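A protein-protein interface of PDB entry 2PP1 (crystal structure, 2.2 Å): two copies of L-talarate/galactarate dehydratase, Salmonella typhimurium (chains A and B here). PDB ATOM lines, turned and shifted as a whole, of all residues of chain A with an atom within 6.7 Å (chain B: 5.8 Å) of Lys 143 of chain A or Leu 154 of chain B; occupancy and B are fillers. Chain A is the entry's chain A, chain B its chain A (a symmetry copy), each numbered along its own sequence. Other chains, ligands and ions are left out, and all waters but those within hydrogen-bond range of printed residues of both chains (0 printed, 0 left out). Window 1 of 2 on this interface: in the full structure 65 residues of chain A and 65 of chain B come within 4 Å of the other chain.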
ATOM      1  N   GLU A  74       0.719 -21.013  -0.209  1.00  0.00           N
ATOM      2  CA  GLU A  74      -0.581 -20.690   0.363  1.00  0.00           C
ATOM      3  C   GLU A  74      -0.465 -19.487   1.281  1.00  0.00           C
ATOM      4  O   GLU A  74       0.579 -19.254   1.884  1.00  0.00           O
ATOM      5  CB  GLU A  74      -1.146 -21.888   1.132  1.00  0.00           C
ATOM      6  CG  GLU A  74      -1.177 -21.739   2.662  1.00  0.00           C
ATOM      7  CD  GLU A  74       0.203 -21.713   3.266  1.00  0.00           C
ATOM      8  OE1 GLU A  74       1.165 -22.009   2.528  1.00  0.00           O
ATOM      9  OE2 GLU A  74       0.329 -21.404   4.468  1.00  0.00           O
ATOM     10  N   GLY A  75      -1.542 -18.718   1.367  1.00  0.00           N
ATOM     11  CA  GLY A  75      -1.554 -17.550   2.224  1.00  0.00           C
ATOM     12  C   GLY A  75      -2.882 -17.475   2.946  1.00  0.00           C
ATOM     13  O   GLY A  75      -3.920 -17.906   2.421  1.00  0.00           O
ATOM     14  N   PRO A 105       0.116 -13.993  -7.923  1.00  0.00           N
ATOM     15  CA  PRO A 105      -0.028 -13.545  -6.534  1.00  0.00           C
ATOM     16  C   PRO A 105       1.008 -12.555  -6.018  1.00  0.00           C
ATOM     17  O   PRO A 105       0.806 -11.952  -4.967  1.00  0.00           O
ATOM     18  CB  PRO A 105      -0.006 -14.858  -5.744  1.00  0.00           C
ATOM     19  CG  PRO A 105       0.930 -15.708  -6.562  1.00  0.00           C
ATOM     20  CD  PRO A 105       0.482 -15.426  -7.981  1.00  0.00           C
ATOM     21  N   ASN A 106       2.117 -12.389  -6.730  1.00  0.00           N
ATOM     22  CA  ASN A 106       3.139 -11.458  -6.277  1.00  0.00           C
ATOM     23  C   ASN A 106       2.812  -9.997  -6.604  1.00  0.00           C
ATOM     24  O   ASN A 106       3.359  -9.089  -5.979  1.00  0.00           O
ATOM     25  CB  ASN A 106       4.497 -11.823  -6.873  1.00  0.00           C
ATOM     26  CG  ASN A 106       4.958 -13.219  -6.464  1.00  0.00           C
ATOM     27  OD1 ASN A 106       4.976 -14.132  -7.285  1.00  0.00           O
ATOM     28  ND2 ASN A 106       5.319 -13.390  -5.195  1.00  0.00           N
ATOM     29  N   ASP A 107       1.937  -9.775  -7.582  1.00  0.00           N
ATOM     30  CA  ASP A 107       1.547  -8.423  -7.970  1.00  0.00           C
ATOM     31  C   ASP A 107       0.354  -7.986  -7.110  1.00  0.00           C
ATOM     32  O   ASP A 107      -0.758  -7.767  -7.598  1.00  0.00           O
ATOM     33  CB  ASP A 107       1.195  -8.383  -9.460  1.00  0.00           C
ATOM     34  CG  ASP A 107       2.410  -8.636 -10.354  1.00  0.00           C
ATOM     35  OD1 ASP A 107       3.554  -8.514  -9.862  1.00  0.00           O
ATOM     36  OD2 ASP A 107       2.227  -8.942 -11.553  1.00  0.00           O
ATOM     37  N   ILE A 108       0.619  -7.867  -5.817  1.00  0.00           N
ATOM     38  CA  ILE A 108      -0.375  -7.507  -4.823  1.00  0.00           C
ATOM     39  C   ILE A 108      -1.126  -6.208  -5.104  1.00  0.00           C
ATOM     40  O   ILE A 108      -2.353  -6.152  -4.988  1.00  0.00           O
ATOM     41  CB  ILE A 108       0.289  -7.435  -3.447  1.00  0.00           C
ATOM     42  CG1 ILE A 108       0.912  -8.806  -3.132  1.00  0.00           C
ATOM     43  CG2 ILE A 108      -0.731  -7.002  -2.387  1.00  0.00           C
ATOM     44  CD1 ILE A 108       1.532  -8.918  -1.770  1.00  0.00           C
ATOM     45  N   ALA A 138      -3.616 -12.069   2.995  1.00  0.00           N
ATOM     46  CA  ALA A 138      -3.242 -13.434   2.628  1.00  0.00           C
ATOM     47  C   ALA A 138      -2.123 -13.421   1.586  1.00  0.00           C
ATOM     48  O   ALA A 138      -1.210 -14.248   1.636  1.00  0.00           O
ATOM     49  CB  ALA A 138      -4.445 -14.199   2.077  1.00  0.00           C
ATOM     50  N   LEU A 139      -2.193 -12.494   0.640  1.00  0.00           N
ATOM     51  CA  LEU A 139      -1.163 -12.409  -0.385  1.00  0.00           C
ATOM     52  C   LEU A 139       0.186 -12.008   0.223  1.00  0.00           C
ATOM     53  O   LEU A 139       1.226 -12.499  -0.200  1.00  0.00           O
ATOM     54  CB  LEU A 139      -1.579 -11.426  -1.482  1.00  0.00           C
ATOM     55  CG  LEU A 139      -2.792 -11.864  -2.311  1.00  0.00           C
ATOM     56  CD1 LEU A 139      -3.190 -10.759  -3.284  1.00  0.00           C
ATOM     57  CD2 LEU A 139      -2.461 -13.150  -3.064  1.00  0.00           C
ATOM     58  N   TRP A 140       0.178 -11.120   1.215  1.00  0.00           N
ATOM     59  CA  TRP A 140       1.437 -10.737   1.854  1.00  0.00           C
ATOM     60  C   TRP A 140       1.954 -11.932   2.653  1.00  0.00           C
ATOM     61  O   TRP A 140       3.153 -12.201   2.690  1.00  0.00           O
ATOM     62  CB  TRP A 140       1.248  -9.541   2.792  1.00  0.00           C
ATOM     63  CG  TRP A 140       1.307  -8.214   2.087  1.00  0.00           C
ATOM     64  CD1 TRP A 140       0.251  -7.457   1.664  1.00  0.00           C
ATOM     65  CD2 TRP A 140       2.493  -7.516   1.685  1.00  0.00           C
ATOM     66  NE1 TRP A 140       0.706  -6.328   1.020  1.00  0.00           N
ATOM     67  CE2 TRP A 140       2.080  -6.339   1.021  1.00  0.00           C
ATOM     68  CE3 TRP A 140       3.868  -7.773   1.821  1.00  0.00           C
ATOM     69  CZ2 TRP A 140       2.994  -5.411   0.493  1.00  0.00           C
ATOM     70  CZ3 TRP A 140       4.782  -6.851   1.296  1.00  0.00           C
ATOM     71  CH2 TRP A 140       4.338  -5.683   0.640  1.00  0.00           C
ATOM     72  N   ASP A 141       1.036 -12.634   3.301  1.00  0.00           N
ATOM     73  CA  ASP A 141       1.375 -13.806   4.095  1.00  0.00           C
ATOM     74  C   ASP A 141       2.074 -14.805   3.162  1.00  0.00           C
ATOM     75  O   ASP A 141       3.112 -15.379   3.499  1.00  0.00           O
ATOM     76  CB  ASP A 141       0.092 -14.415   4.685  1.00  0.00           C
ATOM     77  CG  ASP A 141       0.343 -15.736   5.417  1.00  0.00           C
ATOM     78  OD1 ASP A 141       1.063 -15.745   6.439  1.00  0.00           O
ATOM     79  OD2 ASP A 141      -0.195 -16.766   4.968  1.00  0.00           O
ATOM     80  N   MET A 142       1.503 -14.980   1.974  1.00  0.00           N
ATOM     81  CA  MET A 142       2.058 -15.884   0.981  1.00  0.00           C
ATOM     82  C   MET A 142       3.439 -15.441   0.492  1.00  0.00           C
ATOM     83  O   MET A 142       4.355 -16.256   0.401  1.00  0.00           O
ATOM     84  CB  MET A 142       1.115 -16.006  -0.219  1.00  0.00           C
ATOM     85  CG  MET A 142       1.633 -16.956  -1.294  1.00  0.00           C
ATOM     86  SD  MET A 142       0.674 -16.950  -2.821  1.00  0.00           S
ATOM     87  CE  MET A 142      -0.790 -17.916  -2.300  1.00  0.00           C
ATOM     88  N   LYS A 143       3.599 -14.164   0.170  1.00  0.00           N
ATOM     89  CA  LYS A 143       4.893 -13.700  -0.308  1.00  0.00           C
ATOM     90  C   LYS A 143       5.974 -13.914   0.745  1.00  0.00           C
ATOM     91  O   LYS A 143       7.084 -14.334   0.422  1.00  0.00           O
ATOM     92  CB  LYS A 143       4.838 -12.223  -0.704  1.00  0.00           C
ATOM     93  CG  LYS A 143       6.162 -11.700  -1.257  1.00  0.00           C
ATOM     94  CD  LYS A 143       6.013 -10.327  -1.911  1.00  0.00           C
ATOM     95  CE  LYS A 143       5.244 -10.403  -3.222  1.00  0.00           C
ATOM     96  NZ  LYS A 143       5.131  -9.049  -3.862  1.00  0.00           N
ATOM     97  N   ALA A 144       5.653 -13.630   2.003  1.00  0.00           N
ATOM     98  CA  ALA A 144       6.617 -13.814   3.081  1.00  0.00           C
ATOM     99  C   ALA A 144       7.020 -15.283   3.129  1.00  0.00           C
ATOM    100  O   ALA A 144       8.209 -15.607   3.217  1.00  0.00           O
ATOM    101  CB  ALA A 144       6.010 -13.396   4.414  1.00  0.00           C
ATOM    102  N   LYS A 145       6.027 -16.168   3.075  1.00  0.00           N
ATOM    103  CA  LYS A 145       6.298 -17.605   3.110  1.00  0.00           C
ATOM    104  C   LYS A 145       7.153 -18.017   1.924  1.00  0.00           C
ATOM    105  O   LYS A 145       8.064 -18.827   2.069  1.00  0.00           O
ATOM    106  CB  LYS A 145       4.989 -18.399   3.123  1.00  0.00           C
ATOM    107  CG  LYS A 145       4.316 -18.404   4.484  1.00  0.00           C
ATOM    108  CD  LYS A 145       2.878 -18.895   4.407  1.00  0.00           C
ATOM    109  CE  LYS A 145       2.261 -18.970   5.805  1.00  0.00           C
ATOM    110  NZ  LYS A 145       0.783 -19.185   5.764  1.00  0.00           N
ATOM    111  N   ARG A 146       6.859 -17.455   0.758  1.00  0.00           N
ATOM    112  CA  ARG A 146       7.626 -17.753  -0.444  1.00  0.00           C
ATOM    113  C   ARG A 146       9.106 -17.433  -0.220  1.00  0.00           C
ATOM    114  O   ARG A 146       9.984 -18.108  -0.762  1.00  0.00           O
ATOM    115  CB  ARG A 146       7.091 -16.936  -1.626  1.00  0.00           C
ATOM    116  CG  ARG A 146       7.848 -17.130  -2.936  1.00  0.00           C
ATOM    117  CD  ARG A 146       7.327 -16.168  -4.000  1.00  0.00           C
ATOM    118  NE  ARG A 146       5.913 -16.390  -4.283  1.00  0.00           N
ATOM    119  CZ  ARG A 146       5.441 -17.331  -5.101  1.00  0.00           C
ATOM    120  NH1 ARG A 146       6.278 -18.152  -5.739  1.00  0.00           N
ATOM    121  NH2 ARG A 146       4.125 -17.458  -5.272  1.00  0.00           N
ATOM    122  N   ALA A 147       9.378 -16.407   0.583  1.00  0.00           N
ATOM    123  CA  ALA A 147      10.758 -16.011   0.877  1.00  0.00           C
ATOM    124  C   ALA A 147      11.302 -16.740   2.102  1.00  0.00           C
ATOM    125  O   ALA A 147      12.476 -16.581   2.459  1.00  0.00           O
ATOM    126  CB  ALA A 147      10.832 -14.498   1.106  1.00  0.00           C
ATOM    127  N   GLY A 148      10.449 -17.530   2.750  1.00  0.00           N
ATOM    128  CA  GLY A 148      10.863 -18.250   3.943  1.00  0.00           C
ATOM    129  C   GLY A 148      11.163 -17.296   5.092  1.00  0.00           C
ATOM    130  O   GLY A 148      12.138 -17.474   5.821  1.00  0.00           O
ATOM    131  N   LEU A 149      10.321 -16.281   5.262  1.00  0.00           N
ATOM    132  CA  LEU A 149      10.531 -15.286   6.313  1.00  0.00           C
ATOM    133  C   LEU A 149       9.269 -14.881   7.045  1.00  0.00           C
ATOM    134  O   LEU A 149       8.170 -14.949   6.504  1.00  0.00           O
ATOM    135  CB  LEU A 149      11.097 -13.995   5.724  1.00  0.00           C
ATOM    136  CG  LEU A 149      12.378 -13.908   4.904  1.00  0.00           C
ATOM    137  CD1 LEU A 149      12.456 -12.508   4.255  1.00  0.00           C
ATOM    138  CD2 LEU A 149      13.578 -14.162   5.799  1.00  0.00           C
ATOM    139  N   LEU A 151       6.598 -12.364   8.262  1.00  0.00           N
ATOM    140  CA  LEU A 151       6.227 -11.149   7.534  1.00  0.00           C
ATOM    141  C   LEU A 151       7.097  -9.935   7.899  1.00  0.00           C
ATOM    142  O   LEU A 151       7.521  -9.192   7.020  1.00  0.00           O
ATOM    143  CB  LEU A 151       4.758 -10.812   7.770  1.00  0.00           C
ATOM    144  CG  LEU A 151       4.243  -9.560   7.054  1.00  0.00           C
ATOM    145  CD1 LEU A 151       4.425  -9.696   5.542  1.00  0.00           C
ATOM    146  CD2 LEU A 151       2.760  -9.369   7.402  1.00  0.00           C
ATOM    147  N   LEU A 154      10.161  -9.925   5.895  1.00  0.00           N
ATOM    148  CA  LEU A 154       9.961  -9.666   4.483  1.00  0.00           C
ATOM    149  C   LEU A 154       9.884  -8.137   4.314  1.00  0.00           C
ATOM    150  O   LEU A 154      10.479  -7.571   3.396  1.00  0.00           O
ATOM    151  CB  LEU A 154       8.653 -10.300   3.985  1.00  0.00           C
ATOM    152  CG  LEU A 154       8.184  -9.826   2.592  1.00  0.00           C
ATOM    153  CD1 LEU A 154       9.157 -10.283   1.538  1.00  0.00           C
ATOM    154  CD2 LEU A 154       6.789 -10.363   2.284  1.00  0.00           C
ATOM    155  N   GLY A 375       5.607 -15.808   7.244  1.00  0.00           N
ATOM    156  CA  GLY A 375       4.419 -15.003   7.006  1.00  0.00           C
ATOM    157  C   GLY A 375       3.897 -14.486   8.326  1.00  0.00           C
ATOM    158  O   GLY A 375       4.680 -14.076   9.179  1.00  0.00           O
ATOM    159  N   TRP B 140      18.441  -5.656  -1.611  1.00  0.00           N
ATOM    160  CA  TRP B 140      17.137  -5.880  -2.236  1.00  0.00           C
ATOM    161  C   TRP B 140      17.281  -7.007  -3.256  1.00  0.00           C
ATOM    162  O   TRP B 140      16.398  -7.851  -3.400  1.00  0.00           O
ATOM    163  CB  TRP B 140      16.627  -4.619  -2.938  1.00  0.00           C
ATOM    164  CG  TRP B 140      15.920  -3.666  -2.015  1.00  0.00           C
ATOM    165  CD1 TRP B 140      16.445  -2.557  -1.412  1.00  0.00           C
ATOM    166  CD2 TRP B 140      14.566  -3.772  -1.556  1.00  0.00           C
ATOM    167  NE1 TRP B 140      15.501  -1.965  -0.604  1.00  0.00           N
ATOM    168  CE2 TRP B 140      14.337  -2.691  -0.676  1.00  0.00           C
ATOM    169  CE3 TRP B 140      13.522  -4.680  -1.803  1.00  0.00           C
ATOM    170  CZ2 TRP B 140      13.100  -2.486  -0.039  1.00  0.00           C
ATOM    171  CZ3 TRP B 140      12.289  -4.480  -1.171  1.00  0.00           C
ATOM    172  CH2 TRP B 140      12.090  -3.389  -0.298  1.00  0.00           C
ATOM    173  N   LYS B 143      17.168 -10.165  -1.290  1.00  0.00           N
ATOM    174  CA  LYS B 143      15.849 -10.537  -0.803  1.00  0.00           C
ATOM    175  C   LYS B 143      14.987 -11.095  -1.930  1.00  0.00           C
ATOM    176  O   LYS B 143      14.277 -12.081  -1.741  1.00  0.00           O
ATOM    177  CB  LYS B 143      15.144  -9.344  -0.151  1.00  0.00           C
ATOM    178  CG  LYS B 143      13.771  -9.696   0.418  1.00  0.00           C
ATOM    179  CD  LYS B 143      13.215  -8.587   1.310  1.00  0.00           C
ATOM    180  CE  LYS B 143      13.975  -8.480   2.624  1.00  0.00           C
ATOM    181  NZ  LYS B 143      13.397  -7.403   3.497  1.00  0.00           N
ATOM    182  N   ALA B 144      15.049 -10.469  -3.101  1.00  0.00           N
ATOM    183  CA  ALA B 144      14.271 -10.936  -4.241  1.00  0.00           C
ATOM    184  C   ALA B 144      14.691 -12.364  -4.566  1.00  0.00           C
ATOM    185  O   ALA B 144      13.843 -13.240  -4.769  1.00  0.00           O
ATOM    186  CB  ALA B 144      14.502 -10.037  -5.448  1.00  0.00           C
ATOM    187  N   ALA B 147      13.397 -14.981  -2.378  1.00  0.00           N
ATOM    188  CA  ALA B 147      12.000 -15.318  -2.666  1.00  0.00           C
ATOM    189  C   ALA B 147      11.857 -15.995  -4.026  1.00  0.00           C
ATOM    190  O   ALA B 147      10.756 -16.413  -4.408  1.00  0.00           O
ATOM    191  CB  ALA B 147      11.137 -14.053  -2.630  1.00  0.00           C
ATOM    192  N   LEU B 149      12.295 -14.546  -7.003  1.00  0.00           N
ATOM    193  CA  LEU B 149      11.544 -13.639  -7.873  1.00  0.00           C
ATOM    194  C   LEU B 149      12.371 -12.515  -8.458  1.00  0.00           C
ATOM    195  O   LEU B 149      13.369 -12.093  -7.883  1.00  0.00           O
ATOM    196  CB  LEU B 149      10.417 -12.961  -7.095  1.00  0.00           C
ATOM    197  CG  LEU B 149       9.322 -13.701  -6.337  1.00  0.00           C
ATOM    198  CD1 LEU B 149       8.558 -12.687  -5.457  1.00  0.00           C
ATOM    199  CD2 LEU B 149       8.388 -14.382  -7.322  1.00  0.00           C
ATOM    200  N   PRO B 150      11.984 -12.042  -9.643  1.00  0.00           N
ATOM    201  CA  PRO B 150      12.725 -10.923 -10.232  1.00  0.00           C
ATOM    202  C   PRO B 150      12.400  -9.792  -9.225  1.00  0.00           C
ATOM    203  O   PRO B 150      11.345  -9.831  -8.570  1.00  0.00           O
ATOM    204  CB  PRO B 150      12.011 -10.709 -11.565  1.00  0.00           C
ATOM    205  CG  PRO B 150      11.563 -12.108 -11.934  1.00  0.00           C
ATOM    206  CD  PRO B 150      11.063 -12.658 -10.615  1.00  0.00           C
ATOM    207  N   LEU B 151      13.271  -8.806  -9.079  1.00  0.00           N
ATOM    208  CA  LEU B 151      12.989  -7.726  -8.131  1.00  0.00           C
ATOM    209  C   LEU B 151      11.596  -7.102  -8.320  1.00  0.00           C
ATOM    210  O   LEU B 151      10.892  -6.858  -7.347  1.00  0.00           O
ATOM    211  CB  LEU B 151      14.053  -6.637  -8.230  1.00  0.00           C
ATOM    212  CG  LEU B 151      13.874  -5.448  -7.281  1.00  0.00           C
ATOM    213  CD1 LEU B 151      13.865  -5.923  -5.827  1.00  0.00           C
ATOM    214  CD2 LEU B 151      15.020  -4.454  -7.515  1.00  0.00           C
ATOM    215  N   ALA B 152      11.203  -6.856  -9.567  1.00  0.00           N
ATOM    216  CA  ALA B 152       9.903  -6.256  -9.856  1.00  0.00           C
ATOM    217  C   ALA B 152       8.763  -7.034  -9.205  1.00  0.00           C
ATOM    218  O   ALA B 152       7.797  -6.446  -8.706  1.00  0.00           O
ATOM    219  CB  ALA B 152       9.692  -6.177 -11.361  1.00  0.00           C
ATOM    220  N   LYS B 153       8.888  -8.358  -9.193  1.00  0.00           N
ATOM    221  CA  LYS B 153       7.865  -9.215  -8.604  1.00  0.00           C
ATOM    222  C   LYS B 153       7.893  -9.202  -7.081  1.00  0.00           C
ATOM    223  O   LYS B 153       6.849  -9.356  -6.439  1.00  0.00           O
ATOM    224  CB  LYS B 153       8.012 -10.642  -9.133  1.00  0.00           C
ATOM    225  CG  LYS B 153       7.623 -10.771 -10.597  1.00  0.00           C
ATOM    226  CD  LYS B 153       6.145 -10.459 -10.794  1.00  0.00           C
ATOM    227  CE  LYS B 153       5.765 -10.505 -12.258  1.00  0.00           C
ATOM    228  NZ  LYS B 153       4.302 -10.400 -12.442  1.00  0.00           N
ATOM    229  N   LEU B 154       9.082  -9.045  -6.502  1.00  0.00           N
ATOM    230  CA  LEU B 154       9.188  -8.972  -5.057  1.00  0.00           C
ATOM    231  C   LEU B 154       8.464  -7.685  -4.618  1.00  0.00           C
ATOM    232  O   LEU B 154       7.708  -7.684  -3.647  1.00  0.00           O
ATOM    233  CB  LEU B 154      10.658  -8.907  -4.614  1.00  0.00           C
ATOM    234  CG  LEU B 154      10.880  -8.511  -3.138  1.00  0.00           C
ATOM    235  CD1 LEU B 154      10.342  -9.585  -2.230  1.00  0.00           C
ATOM    236  CD2 LEU B 154      12.363  -8.285  -2.859  1.00  0.00           C
ATOM    237  N   LEU B 155       8.687  -6.603  -5.358  1.00  0.00           N
ATOM    238  CA  LEU B 155       8.061  -5.315  -5.053  1.00  0.00           C
ATOM    239  C   LEU B 155       6.578  -5.346  -5.402  1.00  0.00           C
ATOM    240  O   LEU B 155       5.764  -4.703  -4.755  1.00  0.00           O
ATOM    241  CB  LEU B 155       8.737  -4.197  -5.853  1.00  0.00           C
ATOM    242  CG  LEU B 155      10.245  -3.994  -5.630  1.00  0.00           C
ATOM    243  CD1 LEU B 155      10.788  -2.997  -6.643  1.00  0.00           C
ATOM    244  CD2 LEU B 155      10.486  -3.499  -4.218  1.00  0.00           C
ATOM    245  N   GLY B 156       6.240  -6.126  -6.423  1.00  0.00           N
ATOM    246  CA  GLY B 156       4.865  -6.192  -6.887  1.00  0.00           C
ATOM    247  C   GLY B 156       4.841  -5.348  -8.147  1.00  0.00           C
ATOM    248  O   GLY B 156       5.119  -4.153  -8.098  1.00  0.00           O
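Of chain B, only Lys 153 (3.1 Å) and Leu 154 (2.9 Å) come within 4 Å of Lys 143 of chain A.
Printed residues of chain A within 4 Å of Leu 154 of chain B: Lys 143 (2.9 Å).
Of the printed residues of chain A, Lys 143 of chain B touches Leu 154.
Printed residues of chain B within 4 Å of Leu 154 of chain A: Lys 143 (2.9 Å).
Printed residues of chain A within 4 Å of Ala 147 of chain B: Arg 146 and Ala 147.
Printed residues of chain B within 4 Å of Ala 147 of chain A: Ala 147.
Of the printed residues of chain B, Arg 146 of chain A touches Ala 147 (3.3 Å) and Leu 149 (3.9 Å).
The nearest printed residue of chain A that does not touch Leu 154 of chain B is Leu 154 of chain A (4.01 Å).
OD2 of Asp 107 of chain A lies within salt-bridge range of NZ of Lys 153 of chain B (2.7 Å).
The side-chain amino group (NZ) of Lys 143 of chain A sits at hydrogen-bond distance from the backbone carbonyl oxygen (O) of Lys 153 of chain B (3.1 Å).
The backbone carbonyl oxygen (O) of Leu 154 of chain B lies within hydrogen-bond range of the side-chain amino group (NZ) of Lys 143 of chain A.
The backbone carbonyl oxygen (O) of Leu 154 of chain A lies within hydrogen-bond range of the side-chain amino group (NZ) of Lys 143 of chain B (2.9 Å).
ND2 of Asn 106 of chain A touches CD1 of Leu 149 of chain B, at 3.3 Å.
Lys 153 of chain B touches Asn 106 of chain A (O to CB, 3.4 Å).
Gly 156 of chain B touches Asn 106 of chain A (CA to O, 3.4 Å).
OD1 of Asp 107 of chain A touches C of Gly 156 of chain B (3.8 Å).
CG of Arg 146 of chain A touches O of Ala 147 of chain B, 3.3 Å away.
Leu 149 of chain B touches Arg 146 of chain A.
CB of Ala 147 of chain A touches CB of Ala 147 of chain B, at 3.8 Å.
NZ of Lys 143 of chain A sits at hydrogen-bond distance from O of Asn 106 of chain A (2.8 Å).
The side-chain amide nitrogen of Asn 106 of chain A sits close to the guanidinium group of Arg 146 of chain A, 3.2 Å away.
The backbone carbonyl oxygen (O) of Ala 144 of chain B sits at hydrogen-bond distance from the backbone NH (N) of Leu 149 of chain B.
Lys 143 of chain A touches Leu 154 of chain B, and with the chains exchanged Leu 154 of chain A touches Lys 143 of chain B.
Ala 147 of chain A touches its own counterpart, Ala 147 of chain B.
Of the 21 printed residues of chain A, 6 touch a printed residue of chain B.
Of the 12 printed residues of chain B, 6 touch a printed residue of chain A.
Among the printed residues, 11 pairs touch across the chains.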
